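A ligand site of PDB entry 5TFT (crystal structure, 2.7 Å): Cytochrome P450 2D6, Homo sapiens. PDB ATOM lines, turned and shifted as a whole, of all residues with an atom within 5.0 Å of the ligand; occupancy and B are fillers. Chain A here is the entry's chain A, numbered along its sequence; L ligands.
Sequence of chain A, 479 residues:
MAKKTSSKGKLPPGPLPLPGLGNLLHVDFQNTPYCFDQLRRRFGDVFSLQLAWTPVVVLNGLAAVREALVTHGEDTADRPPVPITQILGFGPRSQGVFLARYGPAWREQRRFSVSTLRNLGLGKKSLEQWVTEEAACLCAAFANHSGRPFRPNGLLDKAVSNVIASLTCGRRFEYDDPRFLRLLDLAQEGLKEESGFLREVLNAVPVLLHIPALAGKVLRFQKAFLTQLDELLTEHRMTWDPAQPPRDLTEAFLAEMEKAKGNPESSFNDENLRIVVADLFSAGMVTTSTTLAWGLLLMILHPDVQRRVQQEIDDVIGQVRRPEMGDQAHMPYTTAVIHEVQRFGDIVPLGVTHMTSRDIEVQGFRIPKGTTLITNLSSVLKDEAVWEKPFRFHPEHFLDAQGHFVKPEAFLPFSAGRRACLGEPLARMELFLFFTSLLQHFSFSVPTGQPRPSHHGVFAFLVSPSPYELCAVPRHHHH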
ATOM      1  N   LEU A  69     -12.702   5.715  16.738  1.00  0.00           N
ATOM      2  CA  LEU A  69     -12.066   5.375  15.476  1.00  0.00           C
ATOM      3  C   LEU A  69     -13.048   5.025  14.363  1.00  0.00           C
ATOM      4  O   LEU A  69     -12.695   5.075  13.187  1.00  0.00           O
ATOM      5  CB  LEU A  69     -11.088   4.213  15.681  1.00  0.00           C
ATOM      6  CG  LEU A  69      -9.941   4.470  16.657  1.00  0.00           C
ATOM      7  CD1 LEU A  69      -8.951   3.326  16.617  1.00  0.00           C
ATOM      8  CD2 LEU A  69      -9.261   5.799  16.364  1.00  0.00           C
ATOM      9  N   ARG A  79      -2.956  12.680  12.525  1.00  0.00           N
ATOM     10  CA  ARG A  79      -1.766  12.351  13.301  1.00  0.00           C
ATOM     11  C   ARG A  79      -1.219  13.585  14.014  1.00  0.00           C
ATOM     12  O   ARG A  79      -1.263  14.690  13.467  1.00  0.00           O
ATOM     13  CB  ARG A  79      -0.681  11.760  12.407  1.00  0.00           C
ATOM     14  CG  ARG A  79      -1.039  10.461  11.715  1.00  0.00           C
ATOM     15  CD  ARG A  79      -1.148   9.317  12.696  1.00  0.00           C
ATOM     16  NE  ARG A  79      -1.322   8.039  12.007  1.00  0.00           N
ATOM     17  CZ  ARG A  79      -1.761   6.932  12.589  1.00  0.00           C
ATOM     18  NH1 ARG A  79      -1.891   5.811  11.878  1.00  0.00           N
ATOM     19  NH2 ARG A  79      -2.066   6.934  13.879  1.00  0.00           N
ATOM     20  N   VAL A  97       2.757   7.760   4.528  1.00  0.00           N
ATOM     21  CA  VAL A  97       1.451   7.232   4.880  1.00  0.00           C
ATOM     22  C   VAL A  97       1.280   7.185   6.389  1.00  0.00           C
ATOM     23  O   VAL A  97       0.262   7.644   6.916  1.00  0.00           O
ATOM     24  CB  VAL A  97       1.238   5.808   4.312  1.00  0.00           C
ATOM     25  CG1 VAL A  97      -0.119   5.267   4.729  1.00  0.00           C
ATOM     26  CG2 VAL A  97       1.372   5.819   2.799  1.00  0.00           C
ATOM     27  N   PHE A  98       2.272   6.634   7.070  1.00  0.00           N
ATOM     28  CA  PHE A  98       2.198   6.366   8.502  1.00  0.00           C
ATOM     29  C   PHE A  98       2.015   7.635   9.320  1.00  0.00           C
ATOM     30  O   PHE A  98       1.085   7.736  10.126  1.00  0.00           O
ATOM     31  CB  PHE A  98       3.450   5.624   8.952  1.00  0.00           C
ATOM     32  CG  PHE A  98       3.328   4.993  10.314  1.00  0.00           C
ATOM     33  CD1 PHE A  98       2.807   3.723  10.452  1.00  0.00           C
ATOM     34  CD2 PHE A  98       3.740   5.680  11.449  1.00  0.00           C
ATOM     35  CE1 PHE A  98       2.694   3.139  11.704  1.00  0.00           C
ATOM     36  CE2 PHE A  98       3.627   5.095  12.700  1.00  0.00           C
ATOM     37  CZ  PHE A  98       3.107   3.829  12.829  1.00  0.00           C
ATOM     38  N   TRP A 106      -2.397  12.125   2.569  1.00  0.00           N
ATOM     39  CA  TRP A 106      -2.494  10.803   3.174  1.00  0.00           C
ATOM     40  C   TRP A 106      -3.387   9.877   2.371  1.00  0.00           C
ATOM     41  O   TRP A 106      -3.033   8.720   2.137  1.00  0.00           O
ATOM     42  CB  TRP A 106      -3.015  10.895   4.605  1.00  0.00           C
ATOM     43  CG  TRP A 106      -3.449   9.570   5.144  1.00  0.00           C
ATOM     44  CD1 TRP A 106      -2.664   8.596   5.668  1.00  0.00           C
ATOM     45  CD2 TRP A 106      -4.792   9.051   5.192  1.00  0.00           C
ATOM     46  NE1 TRP A 106      -3.423   7.511   6.046  1.00  0.00           N
ATOM     47  CE2 TRP A 106      -4.732   7.771   5.762  1.00  0.00           C
ATOM     48  CE3 TRP A 106      -6.038   9.562   4.799  1.00  0.00           C
ATOM     49  CZ2 TRP A 106      -5.866   6.983   5.960  1.00  0.00           C
ATOM     50  CZ3 TRP A 106      -7.167   8.782   5.000  1.00  0.00           C
ATOM     51  CH2 TRP A 106      -7.073   7.514   5.577  1.00  0.00           C
ATOM     52  N   ARG A 110      -2.561   6.394   0.836  1.00  0.00           N
ATOM     53  CA  ARG A 110      -3.286   5.304   1.479  1.00  0.00           C
ATOM     54  C   ARG A 110      -3.996   4.432   0.448  1.00  0.00           C
ATOM     55  O   ARG A 110      -3.878   3.211   0.465  1.00  0.00           O
ATOM     56  CB  ARG A 110      -4.310   5.864   2.474  1.00  0.00           C
ATOM     57  CG  ARG A 110      -5.281   4.818   3.021  1.00  0.00           C
ATOM     58  CD  ARG A 110      -4.690   4.068   4.189  1.00  0.00           C
ATOM     59  NE  ARG A 110      -5.555   2.965   4.614  1.00  0.00           N
ATOM     60  CZ  ARG A 110      -5.464   2.354   5.784  1.00  0.00           C
ATOM     61  NH1 ARG A 110      -4.555   2.739   6.669  1.00  0.00           N
ATOM     62  NH2 ARG A 110      -6.283   1.354   6.086  1.00  0.00           N
ATOM     63  N   LEU A 117      -1.151  -3.414  -3.149  1.00  0.00           N
ATOM     64  CA  LEU A 117      -1.010  -4.686  -2.443  1.00  0.00           C
ATOM     65  C   LEU A 117      -2.005  -5.691  -3.007  1.00  0.00           C
ATOM     66  O   LEU A 117      -1.680  -6.859  -3.226  1.00  0.00           O
ATOM     67  CB  LEU A 117      -1.229  -4.518  -0.938  1.00  0.00           C
ATOM     68  CG  LEU A 117      -0.115  -3.858  -0.118  1.00  0.00           C
ATOM     69  CD1 LEU A 117      -0.507  -3.795   1.349  1.00  0.00           C
ATOM     70  CD2 LEU A 117       1.199  -4.596  -0.288  1.00  0.00           C
ATOM     71  N   ILE A 164       8.815  -7.870   2.251  1.00  0.00           N
ATOM     72  CA  ILE A 164       8.572  -6.458   1.994  1.00  0.00           C
ATOM     73  C   ILE A 164       9.339  -5.971   0.780  1.00  0.00           C
ATOM     74  O   ILE A 164       8.781  -5.321  -0.110  1.00  0.00           O
ATOM     75  CB  ILE A 164       8.952  -5.598   3.209  1.00  0.00           C
ATOM     76  CG1 ILE A 164       7.984  -5.855   4.366  1.00  0.00           C
ATOM     77  CG2 ILE A 164       8.936  -4.138   2.832  1.00  0.00           C
ATOM     78  CD1 ILE A 164       6.535  -5.561   4.015  1.00  0.00           C
ATOM     79  N   LEU A 280       6.519   1.609   4.489  1.00  0.00           N
ATOM     80  CA  LEU A 280       6.107   0.237   4.241  1.00  0.00           C
ATOM     81  C   LEU A 280       7.160  -0.777   4.665  1.00  0.00           C
ATOM     82  O   LEU A 280       6.839  -1.843   5.187  1.00  0.00           O
ATOM     83  CB  LEU A 280       5.785   0.037   2.757  1.00  0.00           C
ATOM     84  CG  LEU A 280       4.626   0.877   2.208  1.00  0.00           C
ATOM     85  CD1 LEU A 280       4.498   0.698   0.707  1.00  0.00           C
ATOM     86  CD2 LEU A 280       3.330   0.508   2.912  1.00  0.00           C
ATOM     87  N   ALA A 283       7.600  -0.592   8.860  1.00  0.00           N
ATOM     88  CA  ALA A 283       6.361  -0.931   9.578  1.00  0.00           C
ATOM     89  C   ALA A 283       6.014  -2.411   9.493  1.00  0.00           C
ATOM     90  O   ALA A 283       5.496  -2.995  10.453  1.00  0.00           O
ATOM     91  CB  ALA A 283       5.205  -0.092   9.061  1.00  0.00           C
ATOM     92  N   GLY A 284       6.286  -3.019   8.346  1.00  0.00           N
ATOM     93  CA  GLY A 284       5.953  -4.424   8.138  1.00  0.00           C
ATOM     94  C   GLY A 284       7.137  -5.348   8.307  1.00  0.00           C
ATOM     95  O   GLY A 284       7.111  -6.497   7.850  1.00  0.00           O
ATOM     96  N   THR A 287       7.180  -5.522  13.027  1.00  0.00           N
ATOM     97  CA  THR A 287       5.912  -6.004  13.564  1.00  0.00           C
ATOM     98  C   THR A 287       5.697  -7.489  13.271  1.00  0.00           C
ATOM     99  O   THR A 287       5.436  -8.276  14.175  1.00  0.00           O
ATOM    100  CB  THR A 287       4.705  -5.216  13.006  1.00  0.00           C
ATOM    101  OG1 THR A 287       4.767  -5.196  11.572  1.00  0.00           O
ATOM    102  CG2 THR A 287       4.715  -3.798  13.531  1.00  0.00           C
ATOM    103  N   THR A 288       5.792  -7.856  11.988  1.00  0.00           N
ATOM    104  CA  THR A 288       5.556  -9.231  11.579  1.00  0.00           C
ATOM    105  C   THR A 288       6.631 -10.175  12.120  1.00  0.00           C
ATOM    106  O   THR A 288       6.358 -11.335  12.420  1.00  0.00           O
ATOM    107  CB  THR A 288       5.511  -9.353  10.040  1.00  0.00           C
ATOM    108  OG1 THR A 288       4.839  -8.208   9.494  1.00  0.00           O
ATOM    109  CG2 THR A 288       4.781 -10.616   9.625  1.00  0.00           C
ATOM    110  N   THR A 291       5.956 -10.723  15.976  1.00  0.00           N
ATOM    111  CA  THR A 291       4.841 -11.636  16.128  1.00  0.00           C
ATOM    112  C   THR A 291       5.281 -13.080  15.913  1.00  0.00           C
ATOM    113  O   THR A 291       4.924 -13.971  16.693  1.00  0.00           O
ATOM    114  CB  THR A 291       3.703 -11.308  15.148  1.00  0.00           C
ATOM    115  OG1 THR A 291       3.219  -9.986  15.396  1.00  0.00           O
ATOM    116  CG2 THR A 291       2.552 -12.295  15.327  1.00  0.00           C
ATOM    117  N   GLN A 342      -1.138 -13.365  18.308  1.00  0.00           N
ATOM    118  CA  GLN A 342      -1.287 -11.921  18.165  1.00  0.00           C
ATOM    119  C   GLN A 342      -1.974 -11.309  19.377  1.00  0.00           C
ATOM    120  O   GLN A 342      -1.576 -10.239  19.849  1.00  0.00           O
ATOM    121  CB  GLN A 342      -2.066 -11.574  16.890  1.00  0.00           C
ATOM    122  CG  GLN A 342      -1.270 -11.766  15.614  1.00  0.00           C
ATOM    123  CD  GLN A 342      -1.908 -11.065  14.427  1.00  0.00           C
ATOM    124  OE1 GLN A 342      -2.789 -11.601  13.762  1.00  0.00           O
ATOM    125  NE2 GLN A 342      -1.459  -9.847  14.152  1.00  0.00           N
ATOM    126  N   ILE A 347       1.707  -6.929  20.685  1.00  0.00           N
ATOM    127  CA  ILE A 347       2.985  -6.291  20.404  1.00  0.00           C
ATOM    128  C   ILE A 347       2.910  -4.765  20.314  1.00  0.00           C
ATOM    129  O   ILE A 347       3.905  -4.083  20.532  1.00  0.00           O
ATOM    130  CB  ILE A 347       3.609  -6.841  19.110  1.00  0.00           C
ATOM    131  CG1 ILE A 347       2.774  -6.462  17.892  1.00  0.00           C
ATOM    132  CG2 ILE A 347       3.755  -8.353  19.201  1.00  0.00           C
ATOM    133  CD1 ILE A 347       3.453  -6.748  16.576  1.00  0.00           C
ATOM    134  N   VAL A 348       1.729  -4.242  20.005  1.00  0.00           N
ATOM    135  CA  VAL A 348       1.525  -2.791  19.984  1.00  0.00           C
ATOM    136  C   VAL A 348       0.441  -2.411  20.994  1.00  0.00           C
ATOM    137  O   VAL A 348      -0.684  -2.118  20.612  1.00  0.00           O
ATOM    138  CB  VAL A 348       1.128  -2.275  18.588  1.00  0.00           C
ATOM    139  CG1 VAL A 348       1.468  -0.795  18.474  1.00  0.00           C
ATOM    140  CG2 VAL A 348       1.830  -3.062  17.504  1.00  0.00           C
ATOM    141  N   GLY A 351      -1.040   1.055  20.603  1.00  0.00           N
ATOM    142  CA  GLY A 351      -1.289   1.360  19.212  1.00  0.00           C
ATOM    143  C   GLY A 351      -0.412   2.478  18.688  1.00  0.00           C
ATOM    144  O   GLY A 351       0.722   2.667  19.140  1.00  0.00           O
ATOM    145  N   VAL A 352      -0.924   3.224  17.726  1.00  0.00           N
ATOM    146  CA  VAL A 352      -0.254   4.410  17.211  1.00  0.00           C
ATOM    147  C   VAL A 352      -1.139   5.618  17.501  1.00  0.00           C
ATOM    148  O   VAL A 352      -2.347   5.572  17.261  1.00  0.00           O
ATOM    149  CB  VAL A 352       0.041   4.300  15.710  1.00  0.00           C
ATOM    150  CG1 VAL A 352       0.745   5.536  15.203  1.00  0.00           C
ATOM    151  CG2 VAL A 352       0.884   3.064  15.439  1.00  0.00           C
ATOM    152  N   HIS A 354      -3.344   8.906  17.750  1.00  0.00           N
ATOM    153  CA  HIS A 354      -4.218   9.644  16.854  1.00  0.00           C
ATOM    154  C   HIS A 354      -4.320  11.086  17.322  1.00  0.00           C
ATOM    155  O   HIS A 354      -3.702  11.472  18.316  1.00  0.00           O
ATOM    156  CB  HIS A 354      -5.605   9.006  16.788  1.00  0.00           C
ATOM    157  CG  HIS A 354      -5.633   7.678  16.089  1.00  0.00           C
ATOM    158  ND1 HIS A 354      -6.340   7.472  14.920  1.00  0.00           N
ATOM    159  CD2 HIS A 354      -5.028   6.508  16.379  1.00  0.00           C
ATOM    160  CE1 HIS A 354      -6.172   6.224  14.526  1.00  0.00           C
ATOM    161  NE2 HIS A 354      -5.385   5.613  15.388  1.00  0.00           N
ATOM    162  N   LEU A 377      -4.939  -0.581  22.809  1.00  0.00           N
ATOM    163  CA  LEU A 377      -5.283  -1.850  22.179  1.00  0.00           C
ATOM    164  C   LEU A 377      -5.103  -3.013  23.142  1.00  0.00           C
ATOM    165  O   LEU A 377      -5.776  -4.037  23.012  1.00  0.00           O
ATOM    166  CB  LEU A 377      -4.437  -2.062  20.933  1.00  0.00           C
ATOM    167  CG  LEU A 377      -4.612  -1.046  19.802  1.00  0.00           C
ATOM    168  CD1 LEU A 377      -3.727  -1.424  18.616  1.00  0.00           C
ATOM    169  CD2 LEU A 377      -6.067  -0.963  19.377  1.00  0.00           C
ATOM    170  N   PRO A 413      -5.754  -6.217  16.880  1.00  0.00           N
ATOM    171  CA  PRO A 413      -4.322  -5.938  16.928  1.00  0.00           C
ATOM    172  C   PRO A 413      -3.901  -4.913  15.869  1.00  0.00           C
ATOM    173  O   PRO A 413      -2.855  -4.287  16.002  1.00  0.00           O
ATOM    174  CB  PRO A 413      -3.685  -7.302  16.672  1.00  0.00           C
ATOM    175  CG  PRO A 413      -4.685  -8.002  15.810  1.00  0.00           C
ATOM    176  CD  PRO A 413      -6.036  -7.544  16.292  1.00  0.00           C
ATOM    177  N   PHE A 414      -4.723  -4.754  14.839  1.00  0.00           N
ATOM    178  CA  PHE A 414      -4.440  -3.805  13.765  1.00  0.00           C
ATOM    179  C   PHE A 414      -5.266  -2.526  13.924  1.00  0.00           C
ATOM    180  O   PHE A 414      -5.483  -1.808  12.952  1.00  0.00           O
ATOM    181  CB  PHE A 414      -4.720  -4.422  12.392  1.00  0.00           C
ATOM    182  CG  PHE A 414      -3.981  -5.707  12.138  1.00  0.00           C
ATOM    183  CD1 PHE A 414      -4.630  -6.931  12.266  1.00  0.00           C
ATOM    184  CD2 PHE A 414      -2.646  -5.706  11.769  1.00  0.00           C
ATOM    185  CE1 PHE A 414      -3.967  -8.115  12.024  1.00  0.00           C
ATOM    186  CE2 PHE A 414      -1.969  -6.887  11.529  1.00  0.00           C
ATOM    187  CZ  PHE A 414      -2.629  -8.090  11.652  1.00  0.00           C
ATOM    188  N   SER A 415      -5.710  -2.273  15.149  1.00  0.00           N
ATOM    189  CA  SER A 415      -6.567  -1.135  15.473  1.00  0.00           C
ATOM    190  C   SER A 415      -7.865  -1.139  14.661  1.00  0.00           C
ATOM    191  O   SER A 415      -8.313  -2.197  14.220  1.00  0.00           O
ATOM    192  CB  SER A 415      -5.815   0.182  15.247  1.00  0.00           C
ATOM    193  OG  SER A 415      -6.599   1.288  15.652  1.00  0.00           O
ATOM    194  N   ALA A 416      -8.462   0.026  14.475  1.00  0.00           N
ATOM    195  CA  ALA A 416      -9.715   0.132  13.731  1.00  0.00           C
ATOM    196  C   ALA A 416      -9.871   1.500  13.072  1.00  0.00           C
ATOM    197  O   ALA A 416      -9.175   2.455  13.414  1.00  0.00           O
ATOM    198  CB  ALA A 416     -10.896  -0.151  14.639  1.00  0.00           C
ATOM    199  N   ARG A 418     -10.311   4.330   9.727  1.00  0.00           N
ATOM    200  CA  ARG A 418      -9.611   4.736   8.514  1.00  0.00           C
ATOM    201  C   ARG A 418      -8.111   4.491   8.560  1.00  0.00           C
ATOM    202  O   ARG A 418      -7.493   4.177   7.544  1.00  0.00           O
ATOM    203  CB  ARG A 418      -9.884   6.216   8.233  1.00  0.00           C
ATOM    204  CG  ARG A 418     -11.309   6.519   7.813  1.00  0.00           C
ATOM    205  CD  ARG A 418     -11.609   8.009   7.909  1.00  0.00           C
ATOM    206  NE  ARG A 418     -12.821   8.354   7.167  1.00  0.00           N
ATOM    207  CZ  ARG A 418     -14.048   8.262   7.646  1.00  0.00           C
ATOM    208  NH1 ARG A 418     -15.083   8.602   6.889  1.00  0.00           N
ATOM    209  NH2 ARG A 418     -14.255   7.829   8.880  1.00  0.00           N
ATOM    210  N   ARG A 419      -7.521   4.647   9.744  1.00  0.00           N
ATOM    211  CA  ARG A 419      -6.079   4.567   9.907  1.00  0.00           C
ATOM    212  C   ARG A 419      -5.613   3.165  10.262  1.00  0.00           C
ATOM    213  O   ARG A 419      -4.412   2.938  10.461  1.00  0.00           O
ATOM    214  CB  ARG A 419      -5.617   5.551  10.977  1.00  0.00           C
ATOM    215  CG  ARG A 419      -5.565   6.981  10.515  1.00  0.00           C
ATOM    216  CD  ARG A 419      -4.376   7.205   9.611  1.00  0.00           C
ATOM    217  NE  ARG A 419      -4.138   8.625   9.374  1.00  0.00           N
ATOM    218  CZ  ARG A 419      -2.978   9.137   9.002  1.00  0.00           C
ATOM    219  NH1 ARG A 419      -1.930   8.349   8.822  1.00  0.00           N
ATOM    220  NH2 ARG A 419      -2.861  10.444   8.814  1.00  0.00           N
ATOM    221  N   ALA A 420      -6.547   2.226  10.341  1.00  0.00           N
ATOM    222  CA  ALA A 420      -6.222   0.835  10.664  1.00  0.00           C
ATOM    223  C   ALA A 420      -5.159   0.310   9.704  1.00  0.00           C
ATOM    224  O   ALA A 420      -5.099   0.731   8.546  1.00  0.00           O
ATOM    225  CB  ALA A 420      -7.473  -0.032  10.607  1.00  0.00           C
ATOM    226  N   CYS A 421      -4.330  -0.598  10.209  1.00  0.00           N
ATOM    227  CA  CYS A 421      -3.184  -1.122   9.467  1.00  0.00           C
ATOM    228  C   CYS A 421      -3.531  -1.547   8.050  1.00  0.00           C
ATOM    229  O   CYS A 421      -4.391  -2.405   7.835  1.00  0.00           O
ATOM    230  CB  CYS A 421      -2.581  -2.312  10.234  1.00  0.00           C
ATOM    231  SG  CYS A 421      -1.133  -3.067   9.464  1.00  0.00           S
ATOM    232  N   LEU A 422      -2.862  -0.935   7.072  1.00  0.00           N
ATOM    233  CA  LEU A 422      -3.103  -1.259   5.663  1.00  0.00           C
ATOM    234  C   LEU A 422      -2.368  -2.530   5.277  1.00  0.00           C
ATOM    235  O   LEU A 422      -2.599  -3.104   4.215  1.00  0.00           O
ATOM    236  CB  LEU A 422      -2.705  -0.091   4.750  1.00  0.00           C
ATOM    237  CG  LEU A 422      -1.264   0.420   4.636  1.00  0.00           C
ATOM    238  CD1 LEU A 422      -0.383  -0.456   3.764  1.00  0.00           C
ATOM    239  CD2 LEU A 422      -1.242   1.849   4.129  1.00  0.00           C
ATOM    240  N   GLY A 423      -1.459  -2.964   6.151  1.00  0.00           N
ATOM    241  CA  GLY A 423      -0.642  -4.133   5.887  1.00  0.00           C
ATOM    242  C   GLY A 423      -1.241  -5.428   6.387  1.00  0.00           C
ATOM    243  O   GLY A 423      -0.663  -6.495   6.203  1.00  0.00           O
ATOM    244  N   LEU A 426      -1.451  -8.574   4.105  1.00  0.00           N
ATOM    245  CA  LEU A 426      -0.129  -9.151   3.899  1.00  0.00           C
ATOM    246  C   LEU A 426       0.352  -9.846   5.166  1.00  0.00           C
ATOM    247  O   LEU A 426       0.904 -10.952   5.104  1.00  0.00           O
ATOM    248  CB  LEU A 426       0.871  -8.082   3.477  1.00  0.00           C
ATOM    249  CG  LEU A 426       2.307  -8.573   3.340  1.00  0.00           C
ATOM    250  CD1 LEU A 426       2.441  -9.543   2.186  1.00  0.00           C
ATOM    251  CD2 LEU A 426       3.272  -7.399   3.187  1.00  0.00           C
ATOM    252  N   ALA A 427       0.155  -9.198   6.302  1.00  0.00           N
ATOM    253  CA  ALA A 427       0.503  -9.772   7.603  1.00  0.00           C
ATOM    254  C   ALA A 427      -0.145 -11.129   7.807  1.00  0.00           C
ATOM    255  O   ALA A 427       0.519 -12.086   8.208  1.00  0.00           O
ATOM    256  CB  ALA A 427       0.114  -8.815   8.727  1.00  0.00           C
ATOM    257  N   GLU A 430       1.703 -13.601   5.616  1.00  0.00           N
ATOM    258  CA  GLU A 430       3.024 -13.897   6.153  1.00  0.00           C
ATOM    259  C   GLU A 430       2.941 -14.790   7.379  1.00  0.00           C
ATOM    260  O   GLU A 430       3.702 -15.742   7.508  1.00  0.00           O
ATOM    261  CB  GLU A 430       3.766 -12.610   6.514  1.00  0.00           C
ATOM    262  CG  GLU A 430       4.254 -11.804   5.324  1.00  0.00           C
ATOM    263  CD  GLU A 430       5.161 -10.659   5.753  1.00  0.00           C
ATOM    264  OE1 GLU A 430       6.334 -10.929   6.084  1.00  0.00           O
ATOM    265  OE2 GLU A 430       4.702  -9.497   5.758  1.00  0.00           O
ATOM    266  N   LEU A 431       2.021 -14.474   8.281  1.00  0.00           N
ATOM    267  CA  LEU A 431       1.884 -15.218   9.524  1.00  0.00           C
ATOM    268  C   LEU A 431       1.469 -16.665   9.275  1.00  0.00           C
ATOM    269  O   LEU A 431       2.069 -17.578   9.819  1.00  0.00           O
ATOM    270  CB  LEU A 431       0.887 -14.540  10.463  1.00  0.00           C
ATOM    271  CG  LEU A 431       1.351 -13.213  11.049  1.00  0.00           C
ATOM    272  CD1 LEU A 431       0.276 -12.587  11.933  1.00  0.00           C
ATOM    273  CD2 LEU A 431       2.641 -13.393  11.816  1.00  0.00           C
HETATM  274  C1  LIG L   1      -0.676   1.035  11.006  1.00  0.00           C
HETATM  275  C2  LIG L   1      -0.336  -3.048  13.624  1.00  0.00           C
HETATM  276  C3  LIG L   1       2.023  -5.169   9.933  1.00  0.00           C
HETATM  277  C4  LIG L   1       2.072  -0.958   7.538  1.00  0.00           C
HETATM  278  C5  LIG L   1      -0.772   0.133  12.039  1.00  0.00           C
HETATM  279  C6  LIG L   1      -1.345   0.400  13.339  1.00  0.00           C
HETATM  280  C7  LIG L   1      -1.254  -0.716  14.065  1.00  0.00           C
HETATM  281  C8  LIG L   1      -0.626  -1.743  13.259  1.00  0.00           C
HETATM  282  C9  LIG L   1      -1.744  -0.863  15.492  1.00  0.00           C
HETATM  283  C10 LIG L   1      -1.942   1.759  13.775  1.00  0.00           C
HETATM  284  C11 LIG L   1      -3.369   1.880  13.260  1.00  0.00           C
HETATM  285  C12 LIG L   1      -3.946   3.196  13.706  1.00  0.00           C
HETATM  286  O1  LIG L   1      -3.216   4.224  13.643  1.00  0.00           O
HETATM  287  O2  LIG L   1      -5.124   3.221  14.120  1.00  0.00           O
HETATM  288  C13 LIG L   1       0.302  -3.994  12.854  1.00  0.00           C
HETATM  289  C14 LIG L   1       0.535  -5.380  13.200  1.00  0.00           C
HETATM  290  C15 LIG L   1       1.192  -5.976  12.178  1.00  0.00           C
HETATM  291  C16 LIG L   1       1.394  -4.973  11.154  1.00  0.00           C
HETATM  292  C17 LIG L   1       0.098  -5.987  14.517  1.00  0.00           C
HETATM  293  C18 LIG L   1       1.691  -7.431  12.018  1.00  0.00           C
HETATM  294  C19 LIG L   1       1.551  -8.395  12.923  1.00  0.00           C
HETATM  295  C20 LIG L   1       2.177  -4.240   8.924  1.00  0.00           C
HETATM  296  C21 LIG L   1       2.605  -4.496   7.561  1.00  0.00           C
HETATM  297  C22 LIG L   1       2.624  -3.318   6.906  1.00  0.00           C
HETATM  298  C23 LIG L   1       2.198  -2.297   7.825  1.00  0.00           C
HETATM  299  C24 LIG L   1       2.970  -5.865   7.046  1.00  0.00           C
HETATM  300  C25 LIG L   1       2.991  -2.987   5.427  1.00  0.00           C
HETATM  301  C26 LIG L   1       3.273  -3.876   4.469  1.00  0.00           C
HETATM  302  C27 LIG L   1       1.310  -0.043   8.246  1.00  0.00           C
HETATM  303  C28 LIG L   1       1.021   1.322   7.856  1.00  0.00           C
HETATM  304  C29 LIG L   1       0.266   1.872   8.812  1.00  0.00           C
HETATM  305  C30 LIG L   1       0.055   0.872   9.847  1.00  0.00           C
HETATM  306  C31 LIG L   1       1.481   2.007   6.596  1.00  0.00           C
HETATM  307  C32 LIG L   1      -0.297   3.307   8.835  1.00  0.00           C
HETATM  308  C33 LIG L   1      -1.620   3.365   8.080  1.00  0.00           C
HETATM  309  C34 LIG L   1      -2.176   4.770   8.137  1.00  0.00           C
HETATM  310  O3  LIG L   1      -3.203   5.038   7.453  1.00  0.00           O
HETATM  311  O4  LIG L   1      -1.600   5.614   8.874  1.00  0.00           O
HETATM  312  N1  LIG L   1      -0.345  -1.180  12.018  1.00  0.00           N
HETATM  313  N2  LIG L   1       0.852  -3.785  11.598  1.00  0.00           N
HETATM  314  N3  LIG L   1       1.936  -2.881   9.051  1.00  0.00           N
HETATM  315  N4  LIG L   1       0.707  -0.289   9.464  1.00  0.00           N
HETATM  316 FE1  LIG L   1       0.657  -2.101  10.473  1.00  0.00          FE
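The backbone carbonyl oxygen (O) of Val 97 lies close to an oxygen (O4) of the ligand (3.4 Å). CD1 of Phe 98 touches C32 of the ligand, 3.5 Å away. CD1 of Ile 164 touches C26 of the ligand (3.7 Å). Ala 283 touches the ligand (CB to C4, 3.6 Å). Gly 284 touches the ligand (CA to C21, 3.4 Å). OG1 of Thr 287 touches C3 of the ligand (3.2 Å). OG1 of Thr 288 touches C24 of the ligand, at 3.9 Å. OG1 of Thr 291 touches C19 of the ligand, at 3.4 Å. Gln 342 touches the ligand (NE2 to C19, 3.6 Å). Val 352 touches the ligand. Leu 377 touches the ligand. Pro 413 touches the ligand. Phe 414 touches the ligand. Ala 420 touches the ligand. CD2 of Leu 422 touches C31 of the ligand, 3.7 Å away. Gly 423 touches the ligand (CA to C22, 3.5 Å). CD2 of Leu 426 touches C26 of the ligand (3.7 Å). Ala 427 touches the ligand. Hydrophobic or aromatic side chains within 4 Å of the ligand: Phe 98, Trp 106, Ile 164, Ala 283, Val 352, His 354, Leu 377, Phe 414, Leu 422, Leu 426 and Ala 427.
An iron atom (FE1) of the ligand is bound by the side-chain sulfur (SG) of Cys 421, 2.3 Å away. NH1 of Arg 79 lies within salt-bridge range of O1 of the ligand (2.7 Å). An oxygen (O2) of the ligand lies within hydrogen-bond range of a ring nitrogen (NE2) of His 354 (2.7 Å). The guanidinium group (NH1) of Arg 419 is in salt-bridge range of an oxygen (O4) of the ligand, 2.8 Å away. NH1 of Arg 110 is in salt-bridge range of O3 of the ligand (2.8 Å). NE1 of Trp 106 is in hydrogen-bond range of O3 of the ligand (2.9 Å). OG of Ser 415 is in hydrogen-bond range of O2 of the ligand (2.9 Å).
The backbone carbonyl oxygen of Phe 414 sits at hydrogen-bond distance from the backbone NH of Cys 421, 3.2 Å away. The guanidinium group of Arg 79 lies within hydrogen-bond range of the backbone carbonyl oxygen of Phe 98 (3.1 Å). The guanidinium group (NH1) of Arg 419 is in hydrogen-bond range of the backbone carbonyl oxygen (O) of Val 97. The backbone carbonyl oxygen (O) of Ala 420 sits at hydrogen-bond distance from the guanidinium group (NH2) of Arg 110 (2.8 Å). The backbone carbonyl oxygen (O) of Arg 418 sits close to the guanidinium group (NH1) of Arg 110, 3.4 Å away. OG1 of Thr 291 sits at hydrogen-bond distance from O of Thr 287, 3.1 Å away. OG1 of Thr 287 lies within hydrogen-bond range of O of Ala 283. The backbone carbonyl oxygen (O) of Gly 284 lies within hydrogen-bond range of the side-chain hydroxyl (OG1) of Thr 288, 3.3 Å away.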
